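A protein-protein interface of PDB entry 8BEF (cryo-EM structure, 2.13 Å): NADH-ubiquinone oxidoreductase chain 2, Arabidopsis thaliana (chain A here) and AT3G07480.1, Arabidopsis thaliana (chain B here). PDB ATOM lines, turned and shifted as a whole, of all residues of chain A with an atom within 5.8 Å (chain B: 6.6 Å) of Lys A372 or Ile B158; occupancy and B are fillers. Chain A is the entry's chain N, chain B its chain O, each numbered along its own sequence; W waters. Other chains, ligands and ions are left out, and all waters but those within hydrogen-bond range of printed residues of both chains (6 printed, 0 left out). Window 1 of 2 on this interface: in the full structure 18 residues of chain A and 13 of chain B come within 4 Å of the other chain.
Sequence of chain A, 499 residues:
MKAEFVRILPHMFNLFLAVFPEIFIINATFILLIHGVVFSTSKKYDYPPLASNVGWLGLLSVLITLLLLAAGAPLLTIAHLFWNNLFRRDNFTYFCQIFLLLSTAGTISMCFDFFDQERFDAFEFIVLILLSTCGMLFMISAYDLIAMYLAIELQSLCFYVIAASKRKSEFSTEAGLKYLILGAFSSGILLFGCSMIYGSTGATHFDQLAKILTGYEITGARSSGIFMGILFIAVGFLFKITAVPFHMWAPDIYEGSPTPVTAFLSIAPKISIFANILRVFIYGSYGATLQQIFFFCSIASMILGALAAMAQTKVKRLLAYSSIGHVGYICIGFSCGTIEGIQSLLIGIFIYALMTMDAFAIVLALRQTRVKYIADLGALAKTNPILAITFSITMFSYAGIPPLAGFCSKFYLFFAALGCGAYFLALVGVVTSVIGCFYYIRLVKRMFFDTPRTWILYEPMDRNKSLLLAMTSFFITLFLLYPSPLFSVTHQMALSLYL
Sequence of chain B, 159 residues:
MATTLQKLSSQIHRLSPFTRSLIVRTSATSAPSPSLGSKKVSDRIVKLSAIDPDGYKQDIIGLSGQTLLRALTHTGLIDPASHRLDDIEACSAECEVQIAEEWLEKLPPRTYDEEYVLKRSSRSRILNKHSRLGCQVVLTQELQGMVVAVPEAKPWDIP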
ATOM      1  N   PHE A 171      14.078  15.707  24.064  1.00  0.00           N
ATOM      2  CA  PHE A 171      15.217  15.186  24.841  1.00  0.00           C
ATOM      3  C   PHE A 171      16.555  15.379  24.070  1.00  0.00           C
ATOM      4  O   PHE A 171      17.483  15.891  24.619  1.00  0.00           O
ATOM      5  CB  PHE A 171      14.929  13.736  25.283  1.00  0.00           C
ATOM      6  CG  PHE A 171      13.686  13.548  26.105  1.00  0.00           C
ATOM      7  CD1 PHE A 171      13.616  14.047  27.392  1.00  0.00           C
ATOM      8  CD2 PHE A 171      12.582  12.884  25.589  1.00  0.00           C
ATOM      9  CE1 PHE A 171      12.472  13.872  28.155  1.00  0.00           C
ATOM     10  CE2 PHE A 171      11.443  12.696  26.361  1.00  0.00           C
ATOM     11  CZ  PHE A 171      11.395  13.188  27.643  1.00  0.00           C
ATOM     12  N   GLU A 255      21.518  10.613  28.982  1.00  0.00           N
ATOM     13  CA  GLU A 255      20.131  10.175  28.942  1.00  0.00           C
ATOM     14  C   GLU A 255      19.447  10.746  27.690  1.00  0.00           C
ATOM     15  O   GLU A 255      18.828   9.971  27.044  1.00  0.00           O
ATOM     16  CB  GLU A 255      19.401  10.608  30.198  1.00  0.00           C
ATOM     17  CG  GLU A 255      17.911  10.434  30.078  1.00  0.00           C
ATOM     18  CD  GLU A 255      17.153  10.583  31.371  1.00  0.00           C
ATOM     19  OE1 GLU A 255      17.390  11.551  32.069  1.00  0.00           O
ATOM     20  OE2 GLU A 255      16.350   9.740  31.658  1.00  0.00           O
ATOM     21  N   GLY A 256      19.664  12.011  27.357  1.00  0.00           N
ATOM     22  CA  GLY A 256      18.933  12.634  26.265  1.00  0.00           C
ATOM     23  C   GLY A 256      19.403  12.272  24.873  1.00  0.00           C
ATOM     24  O   GLY A 256      18.625  12.394  23.922  1.00  0.00           O
ATOM     25  N   SER A 257      20.652  11.845  24.724  1.00  0.00           N
ATOM     26  CA  SER A 257      21.168  11.477  23.418  1.00  0.00           C
ATOM     27  C   SER A 257      20.574  10.146  22.961  1.00  0.00           C
ATOM     28  O   SER A 257      20.094   9.358  23.778  1.00  0.00           O
ATOM     29  CB  SER A 257      22.692  11.382  23.454  1.00  0.00           C
ATOM     30  OG  SER A 257      23.281  12.626  23.786  1.00  0.00           O
ATOM     31  N   THR A 259      20.597   6.365  22.180  1.00  0.00           N
ATOM     32  CA  THR A 259      21.342   5.369  22.950  1.00  0.00           C
ATOM     33  C   THR A 259      22.651   4.923  22.299  1.00  0.00           C
ATOM     34  O   THR A 259      23.633   4.739  23.036  1.00  0.00           O
ATOM     35  CB  THR A 259      20.434   4.165  23.242  1.00  0.00           C
ATOM     36  OG1 THR A 259      19.186   4.637  23.763  1.00  0.00           O
ATOM     37  CG2 THR A 259      21.079   3.249  24.271  1.00  0.00           C
ATOM     38  N   THR A 313      15.898   5.917  39.111  1.00  0.00           N
ATOM     39  CA  THR A 313      14.917   4.901  38.741  1.00  0.00           C
ATOM     40  C   THR A 313      15.004   4.493  37.276  1.00  0.00           C
ATOM     41  O   THR A 313      14.283   3.584  36.858  1.00  0.00           O
ATOM     42  CB  THR A 313      13.488   5.381  39.041  1.00  0.00           C
ATOM     43  OG1 THR A 313      13.194   6.552  38.271  1.00  0.00           O
ATOM     44  CG2 THR A 313      13.310   5.681  40.524  1.00  0.00           C
ATOM     45  N   LYS A 314      15.860   5.135  36.485  1.00  0.00           N
ATOM     46  CA  LYS A 314      15.981   4.848  35.063  1.00  0.00           C
ATOM     47  C   LYS A 314      17.359   4.277  34.751  1.00  0.00           C
ATOM     48  O   LYS A 314      18.357   4.635  35.383  1.00  0.00           O
ATOM     49  CB  LYS A 314      15.721   6.103  34.228  1.00  0.00           C
ATOM     50  CG  LYS A 314      14.330   6.681  34.436  1.00  0.00           C
ATOM     51  CD  LYS A 314      14.037   7.780  33.440  1.00  0.00           C
ATOM     52  CE  LYS A 314      14.270   9.144  34.053  1.00  0.00           C
ATOM     53  NZ  LYS A 314      14.113  10.224  33.042  1.00  0.00           N
ATOM     54  N   VAL A 315      17.401   3.388  33.756  1.00  0.00           N
ATOM     55  CA  VAL A 315      18.600   2.595  33.495  1.00  0.00           C
ATOM     56  C   VAL A 315      19.753   3.481  33.027  1.00  0.00           C
ATOM     57  O   VAL A 315      20.875   3.391  33.542  1.00  0.00           O
ATOM     58  CB  VAL A 315      18.287   1.487  32.472  1.00  0.00           C
ATOM     59  CG1 VAL A 315      19.520   0.639  32.205  1.00  0.00           C
ATOM     60  CG2 VAL A 315      17.126   0.622  32.957  1.00  0.00           C
ATOM     61  N   LYS A 316      19.484   4.279  31.992  1.00  0.00           N
ATOM     62  CA  LYS A 316      20.547   5.165  31.425  1.00  0.00           C
ATOM     63  C   LYS A 316      21.190   6.091  32.497  1.00  0.00           C
ATOM     64  O   LYS A 316      22.381   6.110  32.565  1.00  0.00           O
ATOM     65  CB  LYS A 316      20.060   5.981  30.245  1.00  0.00           C
ATOM     66  CG  LYS A 316      19.769   5.184  28.989  1.00  0.00           C
ATOM     67  CD  LYS A 316      19.327   6.096  27.900  1.00  0.00           C
ATOM     68  CE  LYS A 316      20.454   6.452  26.964  1.00  0.00           C
ATOM     69  NZ  LYS A 316      20.022   7.394  25.918  1.00  0.00           N
ATOM     70  N   ARG A 367      16.115  -1.798  24.051  1.00  0.00           N
ATOM     71  CA  ARG A 367      15.526  -0.540  23.472  1.00  0.00           C
ATOM     72  C   ARG A 367      14.612  -0.860  22.300  1.00  0.00           C
ATOM     73  O   ARG A 367      13.757  -0.059  22.014  1.00  0.00           O
ATOM     74  CB  ARG A 367      16.549   0.515  23.039  1.00  0.00           C
ATOM     75  CG  ARG A 367      17.174   1.232  24.229  1.00  0.00           C
ATOM     76  CD  ARG A 367      16.182   2.072  25.003  1.00  0.00           C
ATOM     77  NE  ARG A 367      15.649   3.114  24.133  1.00  0.00           N
ATOM     78  CZ  ARG A 367      14.487   3.731  24.299  1.00  0.00           C
ATOM     79  NH1 ARG A 367      13.720   3.446  25.338  1.00  0.00           N
ATOM     80  NH2 ARG A 367      14.105   4.638  23.424  1.00  0.00           N
ATOM     81  N   ARG A 370      11.702  -0.492  24.021  1.00  0.00           N
ATOM     82  CA  ARG A 370      11.626   0.807  24.693  1.00  0.00           C
ATOM     83  C   ARG A 370      11.797   0.694  26.208  1.00  0.00           C
ATOM     84  O   ARG A 370      11.006   1.233  26.983  1.00  0.00           O
ATOM     85  CB  ARG A 370      10.312   1.516  24.352  1.00  0.00           C
ATOM     86  CG  ARG A 370      10.218   2.012  22.934  1.00  0.00           C
ATOM     87  CD  ARG A 370      10.999   3.299  22.765  1.00  0.00           C
ATOM     88  NE  ARG A 370      10.963   3.801  21.397  1.00  0.00           N
ATOM     89  CZ  ARG A 370      11.589   3.241  20.372  1.00  0.00           C
ATOM     90  NH1 ARG A 370      12.341   2.163  20.524  1.00  0.00           N
ATOM     91  NH2 ARG A 370      11.466   3.782  19.165  1.00  0.00           N
ATOM     92  N   VAL A 371      12.850  -0.007  26.637  1.00  0.00           N
ATOM     93  CA  VAL A 371      13.152  -0.059  28.061  1.00  0.00           C
ATOM     94  C   VAL A 371      13.488   1.343  28.551  1.00  0.00           C
ATOM     95  O   VAL A 371      14.266   2.073  27.924  1.00  0.00           O
ATOM     96  CB  VAL A 371      14.282  -1.063  28.348  1.00  0.00           C
ATOM     97  CG1 VAL A 371      15.620  -0.576  27.812  1.00  0.00           C
ATOM     98  CG2 VAL A 371      14.371  -1.341  29.839  1.00  0.00           C
ATOM     99  N   LYS A 372      12.950   1.734  29.675  1.00  0.00           N
ATOM    100  CA  LYS A 372      13.236   3.082  30.245  1.00  0.00           C
ATOM    101  C   LYS A 372      13.485   2.998  31.738  1.00  0.00           C
ATOM    102  O   LYS A 372      14.430   3.583  32.164  1.00  0.00           O
ATOM    103  CB  LYS A 372      12.107   4.058  29.890  1.00  0.00           C
ATOM    104  CG  LYS A 372      12.209   5.482  30.388  1.00  0.00           C
ATOM    105  CD  LYS A 372      10.941   6.242  30.046  1.00  0.00           C
ATOM    106  CE  LYS A 372      10.864   7.578  30.740  1.00  0.00           C
ATOM    107  NZ  LYS A 372       9.668   8.370  30.367  1.00  0.00           N
ATOM    108  N   TYR A 373      12.659   2.258  32.439  1.00  0.00           N
ATOM    109  CA  TYR A 373      12.771   2.213  33.886  1.00  0.00           C
ATOM    110  C   TYR A 373      13.396   0.896  34.328  1.00  0.00           C
ATOM    111  O   TYR A 373      13.294  -0.119  33.638  1.00  0.00           O
ATOM    112  CB  TYR A 373      11.402   2.368  34.555  1.00  0.00           C
ATOM    113  CG  TYR A 373      10.691   3.669  34.252  1.00  0.00           C
ATOM    114  CD1 TYR A 373      10.961   4.818  34.986  1.00  0.00           C
ATOM    115  CD2 TYR A 373       9.736   3.741  33.247  1.00  0.00           C
ATOM    116  CE1 TYR A 373      10.307   6.007  34.718  1.00  0.00           C
ATOM    117  CE2 TYR A 373       9.078   4.923  32.972  1.00  0.00           C
ATOM    118  CZ  TYR A 373       9.366   6.054  33.709  1.00  0.00           C
ATOM    119  OH  TYR A 373       8.712   7.232  33.441  1.00  0.00           O
ATOM    120  N   ILE A 374      14.037   0.927  35.497  1.00  0.00           N
ATOM    121  CA  ILE A 374      14.554  -0.302  36.091  1.00  0.00           C
ATOM    122  C   ILE A 374      13.424  -1.302  36.303  1.00  0.00           C
ATOM    123  O   ILE A 374      13.582  -2.501  36.049  1.00  0.00           O
ATOM    124  CB  ILE A 374      15.298   0.007  37.403  1.00  0.00           C
ATOM    125  CG1 ILE A 374      16.611   0.740  37.114  1.00  0.00           C
ATOM    126  CG2 ILE A 374      15.558  -1.267  38.190  1.00  0.00           C
ATOM    127  CD1 ILE A 374      17.082   1.608  38.257  1.00  0.00           C
ATOM    128  N   ASP A 376      10.962  -1.832  34.506  1.00  0.00           N
ATOM    129  CA  ASP A 376      10.605  -2.484  33.249  1.00  0.00           C
ATOM    130  C   ASP A 376      11.300  -3.831  33.077  1.00  0.00           C
ATOM    131  O   ASP A 376      10.887  -4.623  32.226  1.00  0.00           O
ATOM    132  CB  ASP A 376      10.944  -1.580  32.058  1.00  0.00           C
ATOM    133  CG  ASP A 376      10.072  -0.338  31.988  1.00  0.00           C
ATOM    134  OD1 ASP A 376       8.949  -0.356  32.538  1.00  0.00           O
ATOM    135  OD2 ASP A 376      10.513   0.661  31.378  1.00  0.00           O
ATOM    136  N   SER B  82       3.108   5.178  26.629  1.00  0.00           N
ATOM    137  CA  SER B  82       3.852   6.100  27.476  1.00  0.00           C
ATOM    138  C   SER B  82       3.849   5.693  28.944  1.00  0.00           C
ATOM    139  O   SER B  82       4.661   6.209  29.715  1.00  0.00           O
ATOM    140  CB  SER B  82       3.286   7.513  27.336  1.00  0.00           C
ATOM    141  OG  SER B  82       2.136   7.685  28.146  1.00  0.00           O
ATOM    142  N   ARG B  84       3.276   1.986  30.695  1.00  0.00           N
ATOM    143  CA  ARG B  84       2.902   0.596  30.466  1.00  0.00           C
ATOM    144  C   ARG B  84       2.673  -0.189  31.749  1.00  0.00           C
ATOM    145  O   ARG B  84       1.969  -1.203  31.717  1.00  0.00           O
ATOM    146  CB  ARG B  84       3.967  -0.101  29.615  1.00  0.00           C
ATOM    147  CG  ARG B  84       3.788   0.143  28.120  1.00  0.00           C
ATOM    148  CD  ARG B  84       4.870  -0.518  27.289  1.00  0.00           C
ATOM    149  NE  ARG B  84       6.194   0.015  27.577  1.00  0.00           N
ATOM    150  CZ  ARG B  84       7.323  -0.486  27.094  1.00  0.00           C
ATOM    151  NH1 ARG B  84       7.323  -1.522  26.274  1.00  0.00           N
ATOM    152  NH2 ARG B  84       8.478   0.075  27.435  1.00  0.00           N
ATOM    153  N   SER B  92       6.764   8.967  35.367  1.00  0.00           N
ATOM    154  CA  SER B  92       7.258  10.333  35.262  1.00  0.00           C
ATOM    155  C   SER B  92       6.095  11.295  35.048  1.00  0.00           C
ATOM    156  O   SER B  92       6.187  12.254  34.280  1.00  0.00           O
ATOM    157  CB  SER B  92       8.292  10.462  34.146  1.00  0.00           C
ATOM    158  OG  SER B  92       9.483   9.764  34.465  1.00  0.00           O
ATOM    159  N   GLU B  94       3.415  10.901  33.435  1.00  0.00           N
ATOM    160  CA  GLU B  94       2.674  10.777  32.186  1.00  0.00           C
ATOM    161  C   GLU B  94       1.196  10.502  32.432  1.00  0.00           C
ATOM    162  O   GLU B  94       0.364  10.817  31.576  1.00  0.00           O
ATOM    163  CB  GLU B  94       3.277   9.669  31.318  1.00  0.00           C
ATOM    164  CG  GLU B  94       4.732   9.888  30.935  1.00  0.00           C
ATOM    165  CD  GLU B  94       5.697   9.268  31.926  1.00  0.00           C
ATOM    166  OE1 GLU B  94       5.252   8.837  33.010  1.00  0.00           O
ATOM    167  OE2 GLU B  94       6.902   9.208  31.619  1.00  0.00           O
ATOM    168  N   PRO B 155       6.622  15.039  27.047  1.00  0.00           N
ATOM    169  CA  PRO B 155       7.531  14.133  26.295  1.00  0.00           C
ATOM    170  C   PRO B 155       7.903  12.956  27.205  1.00  0.00           C
ATOM    171  O   PRO B 155       8.160  13.114  28.381  1.00  0.00           O
ATOM    172  CB  PRO B 155       8.750  14.996  25.919  1.00  0.00           C
ATOM    173  CG  PRO B 155       8.682  16.058  26.964  1.00  0.00           C
ATOM    174  CD  PRO B 155       7.213  16.388  27.085  1.00  0.00           C
ATOM    175  N   TRP B 156       7.976  11.807  26.566  1.00  0.00           N
ATOM    176  CA  TRP B 156       8.241  10.618  27.406  1.00  0.00           C
ATOM    177  C   TRP B 156       9.216   9.628  26.778  1.00  0.00           C
ATOM    178  O   TRP B 156       9.747   8.795  27.504  1.00  0.00           O
ATOM    179  CB  TRP B 156       6.871   9.958  27.718  1.00  0.00           C
ATOM    180  CG  TRP B 156       6.144   9.446  26.514  1.00  0.00           C
ATOM    181  CD1 TRP B 156       5.172  10.100  25.819  1.00  0.00           C
ATOM    182  CD2 TRP B 156       6.371   8.205  25.815  1.00  0.00           C
ATOM    183  NE1 TRP B 156       4.771   9.350  24.750  1.00  0.00           N
ATOM    184  CE2 TRP B 156       5.490   8.188  24.714  1.00  0.00           C
ATOM    185  CE3 TRP B 156       7.207   7.100  26.024  1.00  0.00           C
ATOM    186  CZ2 TRP B 156       5.415   7.110  23.837  1.00  0.00           C
ATOM    187  CZ3 TRP B 156       7.143   6.042  25.147  1.00  0.00           C
ATOM    188  CH2 TRP B 156       6.258   6.050  24.068  1.00  0.00           C
ATOM    189  N   ASP B 157       9.391   9.663  25.502  1.00  0.00           N
ATOM    190  CA  ASP B 157      10.150   8.658  24.733  1.00  0.00           C
ATOM    191  C   ASP B 157      11.630   9.035  24.614  1.00  0.00           C
ATOM    192  O   ASP B 157      12.052   9.473  23.617  1.00  0.00           O
ATOM    193  CB  ASP B 157       9.422   8.368  23.421  1.00  0.00           C
ATOM    194  CG  ASP B 157       9.977   7.166  22.678  1.00  0.00           C
ATOM    195  OD1 ASP B 157       9.718   7.067  21.491  1.00  0.00           O
ATOM    196  OD2 ASP B 157      10.682   6.363  23.289  1.00  0.00           O
ATOM    197  N   ILE B 158      12.372   8.708  25.631  1.00  0.00           N
ATOM    198  CA  ILE B 158      13.828   8.999  25.722  1.00  0.00           C
ATOM    199  C   ILE B 158      14.563   8.351  24.542  1.00  0.00           C
ATOM    200  O   ILE B 158      14.330   7.212  24.274  1.00  0.00           O
ATOM    201  CB  ILE B 158      14.293   8.431  27.082  1.00  0.00           C
ATOM    202  CG1 ILE B 158      14.062   9.348  28.292  1.00  0.00           C
ATOM    203  CG2 ILE B 158      15.762   8.035  27.036  1.00  0.00           C
ATOM    204  CD1 ILE B 158      12.782  10.097  28.375  1.00  0.00           C
ATOM    205  N   PRO B 159      15.345   9.117  23.755  1.00  0.00           N
ATOM    206  CA  PRO B 159      16.191   8.543  22.698  1.00  0.00           C
ATOM    207  C   PRO B 159      17.097   7.399  23.196  1.00  0.00           C
ATOM    208  O   PRO B 159      17.802   7.611  24.136  1.00  0.00           O
ATOM    209  CB  PRO B 159      17.050   9.745  22.364  1.00  0.00           C
ATOM    210  CG  PRO B 159      16.090  10.893  22.485  1.00  0.00           C
ATOM    211  CD  PRO B 159      15.411  10.572  23.795  1.00  0.00           C
HETATM  212  O   HOH W   1       7.417   6.548  30.071  1.00  0.00           O
HETATM  213  O   HOH W   2       8.768   1.950  29.601  1.00  0.00           O
HETATM  214  O   HOH W   3      10.393  -1.795  28.446  1.00  0.00           O
HETATM  215  O   HOH W   4       5.623   6.252  32.752  1.00  0.00           O
HETATM  216  O   HOH W   5      11.582   5.338  25.918  1.00  0.00           O
HETATM  217  O   HOH W   6      10.984  10.579  31.904  1.00  0.00           O
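O of Val A371 is in hydrogen-bond range of NH1 of Arg A367 (3.0 Å).
N of Tyr A373 lies within hydrogen-bond range of OD2 of Asp A376 (2.9 Å).
The side-chain hydroxyl (OH) of Tyr A373 lies within hydrogen-bond range of the side-chain amino group (NZ) of Lys A372 (3.4 Å).
The side-chain amino group of Lys A316 lies within hydrogen-bond range of the backbone carbonyl oxygen of Glu A255, at 3.1 Å.
The guanidinium group (NH1) of Arg A370 is in hydrogen-bond range of the backbone carbonyl oxygen (O) of Arg A367 (3.0 Å).
The side-chain carboxylate (OE2) of Glu A255 is in salt-bridge range of the side-chain amino group (NZ) of Lys A314 (2.7 Å).
Printed residues of chain A that touch a printed residue of chain B: Phe A171, Glu A255, Gly A256, Ser A257, Thr A259, Lys A316, Arg A367, Arg A370, Lys A372 and Tyr A373.
Hydrophobic or aromatic side chains of chain A within 4 Å of the printed part of chain B: Phe A171 and Tyr A373.
Printed residues of chain B that touch a printed residue of chain A: Arg B84, Ser B92, Glu B94, Pro B155, Trp B156, Asp B157, Ile B158 and Pro B159.
Among the printed residues, Asp or Glu carboxylates within 4 Å of a Lys or Arg side-chain nitrogen of the other chain: Arg A367 with Asp B157 (3.8 Å), Arg A370 with Asp B157 (3.2 Å) and Lys A372 with Glu B94 (3.1 Å).
Among the printed residues, pairs that only touch across the chains: Phe A171 with Pro B155 (3.3 Å), Phe A171 with Trp B156 (3.6 Å), Phe A171 with Asp B157 (3.8 Å), Phe A171 with Ile B158 (3.5 Å), Phe A171 with Pro B159 (3.5 Å), Glu A255 with Ile B158 (3.6 Å), Glu A255 with Pro B159 (3.9 Å), Gly A256 with Pro B159 (3.3 Å) and Lys A372 with Ile B158 (3.95 Å).
Of the printed residues of chain B, Phe A171 touches Pro B155 (3.3 Å), Trp B156 (3.6 Å), Asp B157 (3.8 Å), Ile B158 (3.5 Å) and Pro B159 (3.5 Å).
Of the printed residues of chain B, Thr A259 touches Pro B159.
Of the printed residues of chain B, Arg A367 touches Asp B157 (3.8 Å) and Ile B158 (2.7 Å).
Of the printed residues of chain A, Trp B156 touches Phe A171 and Lys A372.
Of the printed residues of chain A, Asp B157 touches Phe A171 (3.8 Å), Arg A367 (3.8 Å) and Arg A370 (3.1 Å).
Of chain A, only Phe A171, Glu A255, Arg A367 and Lys A372 come within 4 Å of Ile B158.
The nearest printed residue of chain B that does not touch Arg A370 is Trp B156 (5.3 Å).
Water W4 lies within hydrogen-bond range of the side-chain carboxylate of Glu B94 (2.6 Å), the backbone carbonyl oxygen of Ser B82 (3.2 Å) and the side-chain hydroxyl of Tyr A373 (3.3 Å).
Water W1 lies within hydrogen-bond range of the backbone carbonyl oxygen (O) of Ser B82 (2.8 Å), the side-chain amino group (NZ) of Lys A372 (2.9 Å) and the side-chain carboxylate (OE2) of Glu B94 (3.1 Å).
Water W2 bridges OD2 of Asp A376 and NH2 of Arg B84.
Water W3 lies within hydrogen-bond range of the guanidinium group (NH2) of Arg B84 (2.9 Å) and the backbone carbonyl oxygen (O) of Arg A370 (3.4 Å).
Water W5 lies within hydrogen-bond range of NH1 of Arg A367 (2.9 Å), OD2 of Asp B157 (3.0 Å) and N of Ile B158 (3.5 Å).
Water W6 lies within hydrogen-bond range of NZ of Lys A372 (3.0 Å), OG of Ser B92 (3.1 Å) and NZ of Lys A314 (3.3 Å).
The backbone carbonyl oxygen of Ile B158 is in hydrogen-bond range of the guanidinium group of Arg A367 (2.7 Å).
OG of Ser B92 sits at hydrogen-bond distance from OH of Tyr A373 (2.8 Å).
OD2 of Asp B157 is in salt-bridge range of NE of Arg A370 (3.2 Å).
The side-chain hydroxyl of Thr A259 lies within hydrogen-bond range of the backbone carbonyl oxygen of Pro B159, 3.3 Å away.
NZ of Lys A372 lies within salt-bridge range of OE2 of Glu B94.
The backbone carbonyl oxygen (O) of Ser A257 lies close to the backbone carbonyl oxygen (O) of Pro B159 (2.9 Å).
O of Pro B159 is in hydrogen-bond range of NZ of Lys A316 (2.9 Å).
The backbone carbonyl oxygen (O) of Trp B156 lies within hydrogen-bond range of the side-chain amino group (NZ) of Lys A372.
OH of Tyr A373 is in hydrogen-bond range of OE2 of Glu B94, 3.2 Å away.
NH2 of Arg A367 is in salt-bridge range of OD2 of Asp B157 (3.8 Å).
O of Arg A370 lies within hydrogen-bond range of NH2 of Arg B84 (2.8 Å).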
